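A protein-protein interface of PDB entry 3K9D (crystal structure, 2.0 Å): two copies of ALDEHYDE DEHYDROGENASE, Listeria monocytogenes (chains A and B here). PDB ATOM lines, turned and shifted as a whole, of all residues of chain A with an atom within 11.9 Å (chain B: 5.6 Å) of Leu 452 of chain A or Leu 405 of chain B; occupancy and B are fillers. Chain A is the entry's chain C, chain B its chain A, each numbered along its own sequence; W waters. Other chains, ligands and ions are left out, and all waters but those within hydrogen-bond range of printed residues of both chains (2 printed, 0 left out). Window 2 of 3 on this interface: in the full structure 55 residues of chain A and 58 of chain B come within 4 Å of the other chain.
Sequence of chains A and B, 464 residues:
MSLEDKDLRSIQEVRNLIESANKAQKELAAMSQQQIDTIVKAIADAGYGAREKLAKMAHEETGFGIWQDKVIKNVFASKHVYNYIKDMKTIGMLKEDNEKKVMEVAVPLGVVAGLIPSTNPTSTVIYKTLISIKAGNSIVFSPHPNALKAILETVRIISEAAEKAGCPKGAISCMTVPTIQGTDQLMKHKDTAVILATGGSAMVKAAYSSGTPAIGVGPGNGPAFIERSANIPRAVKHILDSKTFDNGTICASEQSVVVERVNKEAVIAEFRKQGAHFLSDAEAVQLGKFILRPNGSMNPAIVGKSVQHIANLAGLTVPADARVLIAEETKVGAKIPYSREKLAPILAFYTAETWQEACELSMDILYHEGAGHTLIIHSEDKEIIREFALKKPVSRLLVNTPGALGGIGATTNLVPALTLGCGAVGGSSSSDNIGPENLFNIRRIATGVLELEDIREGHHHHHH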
ATOM      1  N   LYS A 100      19.506 -19.609  36.581  1.00  0.00           N
ATOM      2  CA  LYS A 100      19.761 -20.636  35.571  1.00  0.00           C
ATOM      3  C   LYS A 100      18.452 -21.137  34.977  1.00  0.00           C
ATOM      4  O   LYS A 100      18.454 -21.740  33.903  1.00  0.00           O
ATOM      5  CB  LYS A 100      20.545 -21.810  36.156  1.00  0.00           C
ATOM      6  CG  LYS A 100      22.061 -21.624  36.193  1.00  0.00           C
ATOM      7  CD  LYS A 100      22.717 -22.702  37.071  1.00  0.00           C
ATOM      8  CE  LYS A 100      24.137 -23.080  36.626  1.00  0.00           C
ATOM      9  NZ  LYS A 100      24.991 -21.911  36.287  1.00  0.00           N
ATOM     10  N   VAL A 102      16.440 -23.453  36.390  1.00  0.00           N
ATOM     11  CA  VAL A 102      16.389 -24.889  36.605  1.00  0.00           C
ATOM     12  C   VAL A 102      15.791 -25.124  37.993  1.00  0.00           C
ATOM     13  O   VAL A 102      16.269 -24.562  38.992  1.00  0.00           O
ATOM     14  CB  VAL A 102      17.801 -25.509  36.513  1.00  0.00           C
ATOM     15  CG1 VAL A 102      17.822 -26.942  37.020  1.00  0.00           C
ATOM     16  CG2 VAL A 102      18.322 -25.455  35.073  1.00  0.00           C
ATOM     17  N   ARG A 444      15.245 -32.567  37.019  1.00  0.00           N
ATOM     18  CA  ARG A 444      15.492 -31.145  36.773  1.00  0.00           C
ATOM     19  C   ARG A 444      14.552 -30.559  35.737  1.00  0.00           C
ATOM     20  O   ARG A 444      14.321 -31.145  34.684  1.00  0.00           O
ATOM     21  CB  ARG A 444      16.953 -30.894  36.399  1.00  0.00           C
ATOM     22  CG  ARG A 444      17.928 -31.182  37.509  1.00  0.00           C
ATOM     23  CD  ARG A 444      19.208 -31.757  36.929  1.00  0.00           C
ATOM     24  NE  ARG A 444      20.186 -32.162  37.943  1.00  0.00           N
ATOM     25  CZ  ARG A 444      20.462 -33.415  38.307  1.00  0.00           C
ATOM     26  NH1 ARG A 444      19.824 -34.454  37.778  1.00  0.00           N
ATOM     27  NH2 ARG A 444      21.398 -33.632  39.226  1.00  0.00           N
ATOM     28  N   ILE A 445      14.007 -29.391  36.053  1.00  0.00           N
ATOM     29  CA  ILE A 445      12.995 -28.762  35.208  1.00  0.00           C
ATOM     30  C   ILE A 445      13.583 -27.452  34.701  1.00  0.00           C
ATOM     31  O   ILE A 445      13.722 -26.481  35.456  1.00  0.00           O
ATOM     32  CB  ILE A 445      11.645 -28.582  35.953  1.00  0.00           C
ATOM     33  CG1 ILE A 445      11.111 -29.928  36.455  1.00  0.00           C
ATOM     34  CG2 ILE A 445      10.583 -27.977  35.046  1.00  0.00           C
ATOM     35  CD1 ILE A 445      11.413 -30.233  37.928  1.00  0.00           C
ATOM     36  N   ALA A 446      13.968 -27.455  33.424  1.00  0.00           N
ATOM     37  CA  ALA A 446      14.732 -26.346  32.847  1.00  0.00           C
ATOM     38  C   ALA A 446      13.971 -25.591  31.776  1.00  0.00           C
ATOM     39  O   ALA A 446      13.312 -26.205  30.936  1.00  0.00           O
ATOM     40  CB  ALA A 446      16.042 -26.841  32.310  1.00  0.00           C
ATOM     41  N   THR A 447      14.063 -24.257  31.825  1.00  0.00           N
ATOM     42  CA  THR A 447      13.427 -23.375  30.849  1.00  0.00           C
ATOM     43  C   THR A 447      14.444 -23.062  29.749  1.00  0.00           C
ATOM     44  O   THR A 447      15.655 -23.013  30.012  1.00  0.00           O
ATOM     45  CB  THR A 447      12.868 -22.067  31.514  1.00  0.00           C
ATOM     46  OG1 THR A 447      11.976 -22.413  32.583  1.00  0.00           O
ATOM     47  CG2 THR A 447      12.088 -21.194  30.527  1.00  0.00           C
ATOM     48  N   GLY A 448      13.949 -22.885  28.524  1.00  0.00           N
ATOM     49  CA  GLY A 448      14.779 -22.443  27.399  1.00  0.00           C
ATOM     50  C   GLY A 448      15.441 -21.097  27.613  1.00  0.00           C
ATOM     51  O   GLY A 448      14.803 -20.141  28.046  1.00  0.00           O
ATOM     52  N   VAL A 449      16.733 -21.042  27.300  1.00  0.00           N
ATOM     53  CA  VAL A 449      17.548 -19.846  27.495  1.00  0.00           C
ATOM     54  C   VAL A 449      18.110 -19.353  26.145  1.00  0.00           C
ATOM     55  O   VAL A 449      18.302 -18.138  25.938  1.00  0.00           O
ATOM     56  CB  VAL A 449      18.678 -20.136  28.549  1.00  0.00           C
ATOM     57  CG1 VAL A 449      19.762 -19.077  28.532  1.00  0.00           C
ATOM     58  CG2 VAL A 449      18.077 -20.271  29.959  1.00  0.00           C
ATOM     59  N   LEU A 450      18.344 -20.292  25.226  1.00  0.00           N
ATOM     60  CA  LEU A 450      18.836 -19.979  23.868  1.00  0.00           C
ATOM     61  C   LEU A 450      17.946 -20.574  22.770  1.00  0.00           C
ATOM     62  O   LEU A 450      17.134 -21.453  23.036  1.00  0.00           O
ATOM     63  CB  LEU A 450      20.269 -20.497  23.680  1.00  0.00           C
ATOM     64  CG  LEU A 450      21.461 -19.987  24.489  1.00  0.00           C
ATOM     65  CD1 LEU A 450      22.731 -20.617  23.942  1.00  0.00           C
ATOM     66  CD2 LEU A 450      21.572 -18.469  24.454  1.00  0.00           C
ATOM     67  N   GLU A 451      18.101 -20.081  21.542  1.00  0.00           N
ATOM     68  CA  GLU A 451      17.439 -20.667  20.371  1.00  0.00           C
ATOM     69  C   GLU A 451      18.467 -21.453  19.552  1.00  0.00           C
ATOM     70  O   GLU A 451      19.659 -21.262  19.748  1.00  0.00           O
ATOM     71  CB  GLU A 451      16.826 -19.566  19.504  1.00  0.00           C
ATOM     72  CG  GLU A 451      15.755 -18.737  20.194  1.00  0.00           C
ATOM     73  CD  GLU A 451      14.431 -19.469  20.376  1.00  0.00           C
ATOM     74  OE1 GLU A 451      14.039 -20.264  19.489  1.00  0.00           O
ATOM     75  OE2 GLU A 451      13.768 -19.227  21.403  1.00  0.00           O
ATOM     76  N   LEU A 452      18.007 -22.318  18.637  1.00  0.00           N
ATOM     77  CA  LEU A 452      18.886 -23.044  17.705  1.00  0.00           C
ATOM     78  C   LEU A 452      19.809 -22.084  16.946  1.00  0.00           C
ATOM     79  O   LEU A 452      21.002 -22.351  16.834  1.00  0.00           O
ATOM     80  CB  LEU A 452      18.071 -23.873  16.699  1.00  0.00           C
ATOM     81  CG  LEU A 452      18.543 -25.189  16.037  1.00  0.00           C
ATOM     82  CD1 LEU A 452      17.690 -25.483  14.798  1.00  0.00           C
ATOM     83  CD2 LEU A 452      20.037 -25.315  15.701  1.00  0.00           C
ATOM     84  N   GLU A 453      19.260 -20.956  16.488  1.00  0.00           N
ATOM     85  CA  GLU A 453      20.015 -19.903  15.781  1.00  0.00           C
ATOM     86  C   GLU A 453      21.199 -19.348  16.576  1.00  0.00           C
ATOM     87  O   GLU A 453      22.187 -18.914  15.982  1.00  0.00           O
ATOM     88  CB  GLU A 453      19.100 -18.744  15.335  1.00  0.00           C
ATOM     89  CG  GLU A 453      17.774 -19.161  14.702  1.00  0.00           C
ATOM     90  CD  GLU A 453      16.654 -19.276  15.729  1.00  0.00           C
ATOM     91  OE1 GLU A 453      16.059 -18.240  16.104  1.00  0.00           O
ATOM     92  OE2 GLU A 453      16.377 -20.408  16.165  1.00  0.00           O
ATOM     93  N   ASP A 454      21.098 -19.366  17.908  1.00  0.00           N
ATOM     94  CA  ASP A 454      22.201 -18.934  18.781  1.00  0.00           C
ATOM     95  C   ASP A 454      23.333 -19.951  18.840  1.00  0.00           C
ATOM     96  O   ASP A 454      24.498 -19.581  18.937  1.00  0.00           O
ATOM     97  CB  ASP A 454      21.713 -18.645  20.204  1.00  0.00           C
ATOM     98  CG  ASP A 454      20.688 -17.523  20.263  1.00  0.00           C
ATOM     99  OD1 ASP A 454      20.881 -16.474  19.599  1.00  0.00           O
ATOM    100  OD2 ASP A 454      19.686 -17.693  20.993  1.00  0.00           O
ATOM    101  N   ILE A 455      22.993 -21.231  18.776  1.00  0.00           N
ATOM    102  CA  ILE A 455      24.003 -22.270  18.945  1.00  0.00           C
ATOM    103  C   ILE A 455      24.777 -22.599  17.651  1.00  0.00           C
ATOM    104  O   ILE A 455      25.918 -23.054  17.719  1.00  0.00           O
ATOM    105  CB  ILE A 455      23.447 -23.526  19.698  1.00  0.00           C
ATOM    106  CG1 ILE A 455      22.589 -24.409  18.787  1.00  0.00           C
ATOM    107  CG2 ILE A 455      22.681 -23.096  20.963  1.00  0.00           C
ATOM    108  CD1 ILE A 455      21.913 -25.561  19.499  1.00  0.00           C
ATOM    109  N   ARG A 456      24.167 -22.362  16.487  1.00  0.00           N
ATOM    110  CA  ARG A 456      24.901 -22.454  15.209  1.00  0.00           C
ATOM    111  C   ARG A 456      25.472 -21.120  14.708  1.00  0.00           C
ATOM    112  O   ARG A 456      25.718 -20.951  13.507  1.00  0.00           O
ATOM    113  CB  ARG A 456      24.095 -23.152  14.101  1.00  0.00           C
ATOM    114  CG  ARG A 456      22.607 -22.894  14.064  1.00  0.00           C
ATOM    115  CD  ARG A 456      22.068 -23.126  12.646  1.00  0.00           C
ATOM    116  NE  ARG A 456      20.646 -23.464  12.642  1.00  0.00           N
ATOM    117  CZ  ARG A 456      19.662 -22.628  12.320  1.00  0.00           C
ATOM    118  NH1 ARG A 456      19.926 -21.378  11.955  1.00  0.00           N
ATOM    119  NH2 ARG A 456      18.406 -23.049  12.359  1.00  0.00           N
ATOM    120  N   GLU A 457      25.680 -20.186  15.636  1.00  0.00           N
ATOM    121  CA  GLU A 457      26.333 -18.913  15.338  1.00  0.00           C
ATOM    122  C   GLU A 457      27.460 -18.611  16.333  1.00  0.00           C
ATOM    123  O   GLU A 457      27.595 -19.278  17.370  1.00  0.00           O
ATOM    124  CB  GLU A 457      25.312 -17.771  15.316  1.00  0.00           C
ATOM    125  CG  GLU A 457      25.838 -16.472  14.686  1.00  0.00           C
ATOM    126  CD  GLU A 457      25.022 -15.238  15.065  1.00  0.00           C
ATOM    127  OE1 GLU A 457      23.796 -15.362  15.289  1.00  0.00           O
ATOM    128  OE2 GLU A 457      25.613 -14.136  15.134  1.00  0.00           O
ATOM    129  N   ILE B  72      27.073 -29.250  14.355  1.00  0.00           N
ATOM    130  CA  ILE B  72      26.588 -28.629  15.601  1.00  0.00           C
ATOM    131  C   ILE B  72      26.739 -29.568  16.827  1.00  0.00           C
ATOM    132  O   ILE B  72      27.139 -29.128  17.913  1.00  0.00           O
ATOM    133  CB  ILE B  72      25.114 -28.136  15.432  1.00  0.00           C
ATOM    134  CG1 ILE B  72      25.038 -27.002  14.394  1.00  0.00           C
ATOM    135  CG2 ILE B  72      24.511 -27.646  16.750  1.00  0.00           C
ATOM    136  CD1 ILE B  72      23.664 -26.851  13.769  1.00  0.00           C
ATOM    137  N   LYS B 237       7.805 -23.742  16.481  1.00  0.00           N
ATOM    138  CA  LYS B 237       9.192 -23.560  16.000  1.00  0.00           C
ATOM    139  C   LYS B 237      10.169 -24.405  16.817  1.00  0.00           C
ATOM    140  O   LYS B 237      11.045 -25.049  16.260  1.00  0.00           O
ATOM    141  CB  LYS B 237       9.591 -22.081  16.069  1.00  0.00           C
ATOM    142  CG  LYS B 237      11.008 -21.750  15.635  1.00  0.00           C
ATOM    143  CD  LYS B 237      11.405 -20.363  16.129  1.00  0.00           C
ATOM    144  CE  LYS B 237      12.867 -20.063  15.812  1.00  0.00           C
ATOM    145  NZ  LYS B 237      13.816 -20.867  16.659  1.00  0.00           N
ATOM    146  N   ASP B 241      12.290 -27.356  15.443  1.00  0.00           N
ATOM    147  CA  ASP B 241      13.762 -27.191  15.577  1.00  0.00           C
ATOM    148  C   ASP B 241      14.420 -28.462  16.092  1.00  0.00           C
ATOM    149  O   ASP B 241      15.487 -28.861  15.616  1.00  0.00           O
ATOM    150  CB  ASP B 241      14.133 -26.038  16.531  1.00  0.00           C
ATOM    151  CG  ASP B 241      14.036 -24.656  15.881  1.00  0.00           C
ATOM    152  OD1 ASP B 241      13.911 -24.564  14.644  1.00  0.00           O
ATOM    153  OD2 ASP B 241      14.084 -23.651  16.622  1.00  0.00           O
ATOM    154  N   SER B 242      13.767 -29.076  17.078  1.00  0.00           N
ATOM    155  CA  SER B 242      14.253 -30.294  17.727  1.00  0.00           C
ATOM    156  C   SER B 242      13.942 -31.567  16.943  1.00  0.00           C
ATOM    157  O   SER B 242      14.817 -32.402  16.718  1.00  0.00           O
ATOM    158  CB  SER B 242      13.673 -30.363  19.144  1.00  0.00           C
ATOM    159  OG  SER B 242      13.424 -31.684  19.561  1.00  0.00           O
ATOM    160  N   PHE B 245      15.940 -31.868  13.786  1.00  0.00           N
ATOM    161  CA  PHE B 245      17.384 -31.815  14.016  1.00  0.00           C
ATOM    162  C   PHE B 245      18.054 -33.180  13.835  1.00  0.00           C
ATOM    163  O   PHE B 245      17.788 -34.107  14.598  1.00  0.00           O
ATOM    164  CB  PHE B 245      17.707 -31.260  15.410  1.00  0.00           C
ATOM    165  CG  PHE B 245      19.156 -30.893  15.590  1.00  0.00           C
ATOM    166  CD1 PHE B 245      19.654 -29.702  15.066  1.00  0.00           C
ATOM    167  CD2 PHE B 245      20.019 -31.730  16.268  1.00  0.00           C
ATOM    168  CE1 PHE B 245      20.981 -29.359  15.218  1.00  0.00           C
ATOM    169  CE2 PHE B 245      21.361 -31.389  16.420  1.00  0.00           C
ATOM    170  CZ  PHE B 245      21.832 -30.203  15.897  1.00  0.00           C
ATOM    171  N   ILE B 250      18.367 -37.590  18.122  1.00  0.00           N
ATOM    172  CA  ILE B 250      18.587 -37.323  19.537  1.00  0.00           C
ATOM    173  C   ILE B 250      17.368 -37.802  20.333  1.00  0.00           C
ATOM    174  O   ILE B 250      16.232 -37.523  19.953  1.00  0.00           O
ATOM    175  CB  ILE B 250      18.925 -35.814  19.757  1.00  0.00           C
ATOM    176  CG1 ILE B 250      20.276 -35.481  19.088  1.00  0.00           C
ATOM    177  CG2 ILE B 250      18.979 -35.447  21.253  1.00  0.00           C
ATOM    178  CD1 ILE B 250      20.640 -34.013  19.105  1.00  0.00           C
ATOM    179  N   THR B 401      11.231 -24.763  25.138  1.00  0.00           N
ATOM    180  CA  THR B 401      12.529 -25.004  24.524  1.00  0.00           C
ATOM    181  C   THR B 401      12.346 -26.191  23.589  1.00  0.00           C
ATOM    182  O   THR B 401      11.405 -26.963  23.779  1.00  0.00           O
ATOM    183  CB  THR B 401      13.665 -25.220  25.620  1.00  0.00           C
ATOM    184  OG1 THR B 401      14.965 -24.920  25.074  1.00  0.00           O
ATOM    185  CG2 THR B 401      13.645 -26.619  26.231  1.00  0.00           C
ATOM    186  N   PRO B 402      13.195 -26.307  22.549  1.00  0.00           N
ATOM    187  CA  PRO B 402      13.234 -27.528  21.730  1.00  0.00           C
ATOM    188  C   PRO B 402      13.668 -28.746  22.555  1.00  0.00           C
ATOM    189  O   PRO B 402      14.657 -28.670  23.277  1.00  0.00           O
ATOM    190  CB  PRO B 402      14.308 -27.225  20.674  1.00  0.00           C
ATOM    191  CG  PRO B 402      14.681 -25.809  20.822  1.00  0.00           C
ATOM    192  CD  PRO B 402      14.137 -25.270  22.075  1.00  0.00           C
ATOM    193  N   GLY B 403      12.941 -29.856  22.432  1.00  0.00           N
ATOM    194  CA  GLY B 403      13.221 -31.083  23.209  1.00  0.00           C
ATOM    195  C   GLY B 403      14.631 -31.645  23.111  1.00  0.00           C
ATOM    196  O   GLY B 403      15.266 -31.884  24.125  1.00  0.00           O
ATOM    197  N   ALA B 404      15.115 -31.848  21.889  1.00  0.00           N
ATOM    198  CA  ALA B 404      16.436 -32.430  21.632  1.00  0.00           C
ATOM    199  C   ALA B 404      17.553 -31.564  22.196  1.00  0.00           C
ATOM    200  O   ALA B 404      18.486 -32.060  22.826  1.00  0.00           O
ATOM    201  CB  ALA B 404      16.641 -32.600  20.132  1.00  0.00           C
ATOM    202  N   LEU B 405      17.413 -30.263  21.962  1.00  0.00           N
ATOM    203  CA  LEU B 405      18.390 -29.256  22.282  1.00  0.00           C
ATOM    204  C   LEU B 405      18.308 -28.850  23.759  1.00  0.00           C
ATOM    205  O   LEU B 405      19.310 -28.518  24.368  1.00  0.00           O
ATOM    206  CB  LEU B 405      18.168 -28.041  21.367  1.00  0.00           C
ATOM    207  CG  LEU B 405      18.746 -27.947  19.943  1.00  0.00           C
ATOM    208  CD1 LEU B 405      18.834 -29.263  19.166  1.00  0.00           C
ATOM    209  CD2 LEU B 405      17.928 -26.925  19.140  1.00  0.00           C
ATOM    210  N   GLY B 406      17.114 -28.872  24.335  1.00  0.00           N
ATOM    211  CA  GLY B 406      16.979 -28.539  25.748  1.00  0.00           C
ATOM    212  C   GLY B 406      17.388 -29.678  26.671  1.00  0.00           C
ATOM    213  O   GLY B 406      17.990 -29.443  27.722  1.00  0.00           O
ATOM    214  N   GLY B 407      17.086 -30.910  26.257  1.00  0.00           N
ATOM    215  CA  GLY B 407      17.365 -32.126  27.053  1.00  0.00           C
ATOM    216  C   GLY B 407      18.837 -32.430  27.224  1.00  0.00           C
ATOM    217  O   GLY B 407      19.265 -32.924  28.278  1.00  0.00           O
ATOM    218  N   ILE B 408      19.618 -32.117  26.193  1.00  0.00           N
ATOM    219  CA  ILE B 408      21.070 -32.258  26.252  1.00  0.00           C
ATOM    220  C   ILE B 408      21.784 -31.068  26.925  1.00  0.00           C
ATOM    221  O   ILE B 408      22.974 -31.132  27.174  1.00  0.00           O
ATOM    222  CB  ILE B 408      21.704 -32.612  24.853  1.00  0.00           C
ATOM    223  CG1 ILE B 408      21.732 -31.410  23.897  1.00  0.00           C
ATOM    224  CG2 ILE B 408      21.031 -33.869  24.237  1.00  0.00           C
ATOM    225  CD1 ILE B 408      22.351 -31.721  22.527  1.00  0.00           C
ATOM    226  N   GLY B 409      21.057 -29.990  27.213  1.00  0.00           N
ATOM    227  CA  GLY B 409      21.667 -28.796  27.807  1.00  0.00           C
ATOM    228  C   GLY B 409      22.316 -27.825  26.821  1.00  0.00           C
ATOM    229  O   GLY B 409      23.237 -27.081  27.181  1.00  0.00           O
ATOM    230  N   ALA B 410      21.844 -27.831  25.573  1.00  0.00           N
ATOM    231  CA  ALA B 410      22.365 -26.911  24.557  1.00  0.00           C
ATOM    232  C   ALA B 410      21.563 -25.603  24.542  1.00  0.00           C
ATOM    233  O   ALA B 410      22.134 -24.523  24.438  1.00  0.00           O
ATOM    234  CB  ALA B 410      22.380 -27.570  23.180  1.00  0.00           C
ATOM    235  N   THR B 411      20.241 -25.715  24.662  1.00  0.00           N
ATOM    236  CA  THR B 411      19.380 -24.536  24.815  1.00  0.00           C
ATOM    237  C   THR B 411      18.855 -24.331  26.245  1.00  0.00           C
ATOM    238  O   THR B 411      18.147 -23.353  26.509  1.00  0.00           O
ATOM    239  CB  THR B 411      18.183 -24.532  23.834  1.00  0.00           C
ATOM    240  OG1 THR B 411      17.342 -25.656  24.094  1.00  0.00           O
ATOM    241  CG2 THR B 411      18.651 -24.551  22.393  1.00  0.00           C
ATOM    242  N   THR B 412      19.199 -25.235  27.158  1.00  0.00           N
ATOM    243  CA  THR B 412      18.901 -25.033  28.591  1.00  0.00           C
ATOM    244  C   THR B 412      20.158 -24.950  29.458  1.00  0.00           C
ATOM    245  O   THR B 412      21.266 -25.241  29.009  1.00  0.00           O
ATOM    246  CB  THR B 412      17.993 -26.142  29.179  1.00  0.00           C
ATOM    247  OG1 THR B 412      18.608 -27.436  29.026  1.00  0.00           O
ATOM    248  CG2 THR B 412      16.603 -26.120  28.552  1.00  0.00           C
HETATM  249  O   HOH W   1      14.953 -22.382  23.846  1.00  0.00           O
HETATM  250  O   HOH W   2      15.213 -22.894  18.926  1.00  0.00           O
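Leu 452 of chain A touches two residues of chain B. Of the printed residues of chain B, Glu 453 of chain A touches Lys 237 and Asp 241. Of the printed residues of chain A, Ile 72 of chain B touches Arg 456 (3.7 Å). Ser 242 of chain B touches none of the printed residues of chain A. No residue of chain A comes within 4 Å of Phe 245 of chain B. No residue of chain A comes within 4 Å of Pro 402 of chain B. Gly 403 of chain B touches none of the printed residues of chain A. No residue of chain A comes within 4 Å of Ala 404 of chain B. Printed residues of chain A within 4 Å of Leu 405 of chain B: Leu 452 and Ile 455. Gly 406 of chain B touches none of the printed residues of chain A. No residue of chain A comes within 4 Å of Gly 407 of chain B. No residue of chain A comes within 4 Å of Gly 409 of chain B. Thr 411 of chain B touches just these residues of chain A: Gly 448, Val 449 and Leu 450. Printed residues of chain A within 4 Å of Thr 412 of chain B: Ala 446 and Thr 447.
The side-chain hydroxyl (OG1) of Thr 401 of chain B sits at hydrogen-bond distance from the side-chain hydroxyl (OG1) of Thr 411 of chain B, at 2.7 Å. The backbone carbonyl oxygen (O) of Leu 405 of chain B is in hydrogen-bond range of the backbone NH (N) of Ala 410 of chain B (2.9 Å). The backbone carbonyl oxygen of Leu 405 of chain B lies within hydrogen-bond range of the backbone NH of Thr 411 of chain B (3.0 Å). The backbone NH (N) of Gly 406 of chain B lies within hydrogen-bond range of the side-chain hydroxyl (OG1) of Thr 411 of chain B, 3.2 Å away. O of Gly 406 of chain B lies within hydrogen-bond range of OG1 of Thr 412 of chain B (2.5 Å). OD2 of Asp 454 of chain A lies within hydrogen-bond range of N of Glu 451 of chain A, at 2.9 Å.
Water W1 bridges the backbone carbonyl oxygen (O) of Leu 450 of chain A and the side-chain hydroxyl (OG1) of Thr 401 of chain B. Water W2 lies within hydrogen-bond range of OD2 of Asp 241 of chain B (2.7 Å), N of Leu 452 of chain A (2.9 Å), OE1 of Glu 451 of chain A (2.9 Å) and NZ of Lys 237 of chain B (3.3 Å).
Of the 16 printed residues of chain A, 10 touch a printed residue of chain B. Hydrophobic or aromatic side chains of chain A that line the printed part of chain B: Ala 446, Val 449, Leu 450, Leu 452 and Ile 455. Along chain A the printed residues that touch a printed residue of chain B span positions 446 to 456. Of the 18 printed residues of chain B, 8 touch a printed residue of chain A. Hydrophobic or aromatic side chains of chain B within 4 Å of the printed part of chain A: Ile 72 and Leu 405.
Thr 412 of chain B touches Ala 446 of chain A (CB to CB, 3.8 Å). Thr 447 of chain A touches Thr 412 of chain B (O to CG2, 3.6 Å). Gly 448 of chain A touches Thr 401 of chain B. CA of Gly 448 of chain A touches O of Thr 411 of chain B, 3.6 Å away. Leu 452 of chain A touches Asp 241 of chain B. Leu 452 of chain A touches Leu 405 of chain B (CG to CD2, 3.6 Å). Glu 453 of chain A touches Asp 241 of chain B (OE2 to OD2, 3.998 Å). Ile 455 of chain A touches Leu 405 of chain B. Ala 410 of chain B touches Ile 455 of chain A. Arg 456 of chain A touches Ile 72 of chain B (CB to CD1, 3.7 Å).
The side-chain carboxylate of Glu 451 of chain A is in salt-bridge range of the side-chain amino group of Lys 237 of chain B (2.9 Å). The side-chain carboxylate of Glu 453 of chain A lies within salt-bridge range of the side-chain amino group of Lys 237 of chain B, 2.6 Å away. N of Val 449 of chain A sits at hydrogen-bond distance from O of Thr 411 of chain B (2.8 Å). O of Thr 411 of chain B sits at hydrogen-bond distance from N of Leu 450 of chain A (3.3 Å).
No position is printed for both chains.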
